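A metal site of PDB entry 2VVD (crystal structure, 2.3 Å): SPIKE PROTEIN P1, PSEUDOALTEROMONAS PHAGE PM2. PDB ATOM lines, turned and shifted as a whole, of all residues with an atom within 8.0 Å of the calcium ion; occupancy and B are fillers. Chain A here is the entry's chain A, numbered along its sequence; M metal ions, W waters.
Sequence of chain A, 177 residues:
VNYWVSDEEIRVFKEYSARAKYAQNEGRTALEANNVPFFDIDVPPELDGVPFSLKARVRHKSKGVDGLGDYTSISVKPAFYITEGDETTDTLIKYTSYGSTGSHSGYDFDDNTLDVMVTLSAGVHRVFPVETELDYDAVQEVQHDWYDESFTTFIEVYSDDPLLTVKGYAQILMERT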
ATOM      1  N   THR A  72      -7.044   8.263 -14.971  1.00  0.00           N
ATOM      2  CA  THR A  72      -5.670   7.866 -15.195  1.00  0.00           C
ATOM      3  C   THR A  72      -5.249   6.853 -14.122  1.00  0.00           C
ATOM      4  O   THR A  72      -5.452   7.090 -12.924  1.00  0.00           O
ATOM      5  CB  THR A  72      -4.734   9.098 -15.177  1.00  0.00           C
ATOM      6  OG1 THR A  72      -5.114   9.973 -16.258  1.00  0.00           O
ATOM      7  CG2 THR A  72      -3.278   8.694 -15.344  1.00  0.00           C
ATOM      8  N   SER A  73      -4.696   5.723 -14.553  1.00  0.00           N
ATOM      9  CA  SER A  73      -4.233   4.698 -13.637  1.00  0.00           C
ATOM     10  C   SER A  73      -2.872   5.073 -13.066  1.00  0.00           C
ATOM     11  O   SER A  73      -1.956   5.415 -13.824  1.00  0.00           O
ATOM     12  CB  SER A  73      -4.123   3.347 -14.352  1.00  0.00           C
ATOM     13  OG  SER A  73      -3.566   2.369 -13.477  1.00  0.00           O
ATOM     14  N   ILE A  74      -2.738   5.026 -11.739  1.00  0.00           N
ATOM     15  CA  ILE A  74      -1.494   5.380 -11.055  1.00  0.00           C
ATOM     16  C   ILE A  74      -0.995   4.248 -10.166  1.00  0.00           C
ATOM     17  O   ILE A  74      -1.626   3.905  -9.159  1.00  0.00           O
ATOM     18  CB  ILE A  74      -1.654   6.665 -10.212  1.00  0.00           C
ATOM     19  CG1 ILE A  74      -1.853   7.884 -11.115  1.00  0.00           C
ATOM     20  CG2 ILE A  74      -0.457   6.864  -9.277  1.00  0.00           C
ATOM     21  CD1 ILE A  74      -0.678   8.180 -12.056  1.00  0.00           C
ATOM     22  N   SER A  75       0.134   3.661 -10.550  1.00  0.00           N
ATOM     23  CA  SER A  75       0.766   2.584  -9.789  1.00  0.00           C
ATOM     24  C   SER A  75       1.526   3.208  -8.615  1.00  0.00           C
ATOM     25  O   SER A  75       2.222   4.218  -8.784  1.00  0.00           O
ATOM     26  CB  SER A  75       1.741   1.794 -10.666  1.00  0.00           C
ATOM     27  OG  SER A  75       1.064   1.098 -11.704  1.00  0.00           O
ATOM     28  N   VAL A  76       1.383   2.581  -7.437  1.00  0.00           N
ATOM     29  CA  VAL A  76       2.012   3.069  -6.198  1.00  0.00           C
ATOM     30  C   VAL A  76       2.682   1.939  -5.413  1.00  0.00           C
ATOM     31  O   VAL A  76       2.271   0.778  -5.460  1.00  0.00           O
ATOM     32  CB  VAL A  76       1.006   3.794  -5.274  1.00  0.00           C
ATOM     33  CG1 VAL A  76       0.479   5.051  -5.936  1.00  0.00           C
ATOM     34  CG2 VAL A  76      -0.135   2.859  -4.879  1.00  0.00           C
ATOM     35  N   THR A 101      -2.705  -0.085  -7.836  1.00  0.00           N
ATOM     36  CA  THR A 101      -2.793   0.520  -9.165  1.00  0.00           C
ATOM     37  C   THR A 101      -4.191   1.064  -9.450  1.00  0.00           C
ATOM     38  O   THR A 101      -5.071   1.018  -8.594  1.00  0.00           O
ATOM     39  CB  THR A 101      -2.344  -0.470 -10.262  1.00  0.00           C
ATOM     40  OG1 THR A 101      -2.199   0.210 -11.514  1.00  0.00           O
ATOM     41  CG2 THR A 101      -3.344  -1.617 -10.411  1.00  0.00           C
ATOM     42  N   GLY A 102      -4.381   1.618 -10.650  1.00  0.00           N
ATOM     43  CA  GLY A 102      -5.649   2.230 -11.047  1.00  0.00           C
ATOM     44  C   GLY A 102      -5.833   3.658 -10.535  1.00  0.00           C
ATOM     45  O   GLY A 102      -4.891   4.269 -10.029  1.00  0.00           O
ATOM     46  N   GLU A 133       7.388   4.429  -6.464  1.00  0.00           N
ATOM     47  CA  GLU A 133       6.957   4.233  -7.849  1.00  0.00           C
ATOM     48  C   GLU A 133       6.601   5.565  -8.497  1.00  0.00           C
ATOM     49  O   GLU A 133       5.698   6.261  -8.040  1.00  0.00           O
ATOM     50  CB  GLU A 133       5.757   3.274  -7.893  1.00  0.00           C
ATOM     51  CG  GLU A 133       5.309   2.850  -9.306  1.00  0.00           C
ATOM     52  CD  GLU A 133       6.206   1.784  -9.948  1.00  0.00           C
ATOM     53  OE1 GLU A 133       7.268   1.466  -9.389  1.00  0.00           O
ATOM     54  OE2 GLU A 133       5.835   1.271 -11.029  1.00  0.00           O
ATOM     55  N   LEU A 134       7.332   5.915  -9.554  1.00  0.00           N
ATOM     56  CA  LEU A 134       7.030   7.084 -10.372  1.00  0.00           C
ATOM     57  C   LEU A 134       6.235   6.624 -11.582  1.00  0.00           C
ATOM     58  O   LEU A 134       6.774   5.977 -12.482  1.00  0.00           O
ATOM     59  CB  LEU A 134       8.327   7.791 -10.811  1.00  0.00           C
ATOM     60  CG  LEU A 134       8.190   9.002 -11.746  1.00  0.00           C
ATOM     61  CD1 LEU A 134       7.472  10.158 -11.072  1.00  0.00           C
ATOM     62  CD2 LEU A 134       9.556   9.454 -12.246  1.00  0.00           C
ATOM     63  N   ASP A 135       4.953   6.942 -11.611  1.00  0.00           N
ATOM     64  CA  ASP A 135       4.065   6.431 -12.647  1.00  0.00           C
ATOM     65  C   ASP A 135       4.268   7.193 -13.952  1.00  0.00           C
ATOM     66  O   ASP A 135       4.304   8.421 -13.962  1.00  0.00           O
ATOM     67  CB  ASP A 135       2.609   6.510 -12.199  1.00  0.00           C
ATOM     68  CG  ASP A 135       1.692   5.728 -13.104  1.00  0.00           C
ATOM     69  OD1 ASP A 135       1.395   4.560 -12.767  1.00  0.00           O
ATOM     70  OD2 ASP A 135       1.273   6.257 -14.150  1.00  0.00           O
ATOM     71  N   TYR A 136       4.386   6.452 -15.048  1.00  0.00           N
ATOM     72  CA  TYR A 136       4.685   7.043 -16.349  1.00  0.00           C
ATOM     73  C   TYR A 136       3.578   7.994 -16.840  1.00  0.00           C
ATOM     74  O   TYR A 136       3.879   8.995 -17.481  1.00  0.00           O
ATOM     75  CB  TYR A 136       4.939   5.940 -17.376  1.00  0.00           C
ATOM     76  CG  TYR A 136       5.411   6.458 -18.707  1.00  0.00           C
ATOM     77  CD1 TYR A 136       6.695   6.991 -18.851  1.00  0.00           C
ATOM     78  CD2 TYR A 136       4.583   6.416 -19.829  1.00  0.00           C
ATOM     79  CE1 TYR A 136       7.144   7.463 -20.080  1.00  0.00           C
ATOM     80  CE2 TYR A 136       5.023   6.885 -21.058  1.00  0.00           C
ATOM     81  CZ  TYR A 136       6.289   7.407 -21.184  1.00  0.00           C
ATOM     82  OH  TYR A 136       6.719   7.870 -22.405  1.00  0.00           O
ATOM     83  N   ASP A 137       2.321   7.686 -16.534  1.00  0.00           N
ATOM     84  CA  ASP A 137       1.210   8.604 -16.861  1.00  0.00           C
ATOM     85  C   ASP A 137       1.364   9.942 -16.153  1.00  0.00           C
ATOM     86  O   ASP A 137       1.082  10.988 -16.720  1.00  0.00           O
ATOM     87  CB  ASP A 137      -0.142   7.987 -16.518  1.00  0.00           C
ATOM     88  CG  ASP A 137      -0.425   6.699 -17.268  1.00  0.00           C
ATOM     89  OD1 ASP A 137      -0.168   6.639 -18.502  1.00  0.00           O
ATOM     90  OD2 ASP A 137      -0.905   5.743 -16.634  1.00  0.00           O
ATOM     91  N   ALA A 138       1.811   9.899 -14.896  1.00  0.00           N
ATOM     92  CA  ALA A 138       2.107  11.107 -14.122  1.00  0.00           C
ATOM     93  C   ALA A 138       3.272  11.876 -14.754  1.00  0.00           C
ATOM     94  O   ALA A 138       3.236  13.109 -14.835  1.00  0.00           O
ATOM     95  CB  ALA A 138       2.441  10.743 -12.685  1.00  0.00           C
ATOM     96  N   GLU A 141       1.624  13.385 -18.026  1.00  0.00           N
ATOM     97  CA  GLU A 141       0.520  14.330 -17.851  1.00  0.00           C
ATOM     98  C   GLU A 141       0.922  15.572 -17.067  1.00  0.00           C
ATOM     99  O   GLU A 141       0.630  16.689 -17.494  1.00  0.00           O
ATOM    100  CB  GLU A 141      -0.671  13.668 -17.148  1.00  0.00           C
ATOM    101  CG  GLU A 141      -1.485  12.738 -18.027  1.00  0.00           C
ATOM    102  CD  GLU A 141      -2.755  12.263 -17.332  1.00  0.00           C
ATOM    103  OE1 GLU A 141      -3.355  13.040 -16.562  1.00  0.00           O
ATOM    104  OE2 GLU A 141      -3.167  11.103 -17.571  1.00  0.00           O
HETATM  105 CA    CA M   1      -0.116   4.326 -14.864  1.00  0.00          CA
HETATM  106  O   HOH W   1      -0.762   2.347 -13.702  1.00  0.00           O
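The side-chain hydroxyl of Ser 73 is in hydrogen-bond range of the side-chain hydroxyl of Thr 101.
The backbone NH (N) of Gly 102 is in hydrogen-bond range of the side-chain hydroxyl (OG) of Ser 73.
The backbone NH of Ser 75 sits close to the side-chain carboxylate of Asp 135 (2.7 Å).
The nearest printed residue that does not touch the calcium ion is Ile 74 (4.1 Å).
The calcium ion is bound by the backbone carbonyl oxygen (O) of Ser 73, water W1, the side-chain carboxylate (OD2) of Asp 137, the side-chain carboxylate (OD2) of Asp 135 and the side-chain carboxylate (OD1) of Asp 135.
The calcium ion has five donor atoms within binding distance.
Water W1 lies within hydrogen-bond range of OG of Ser 73, OG of Ser 75 and OG1 of Thr 101.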
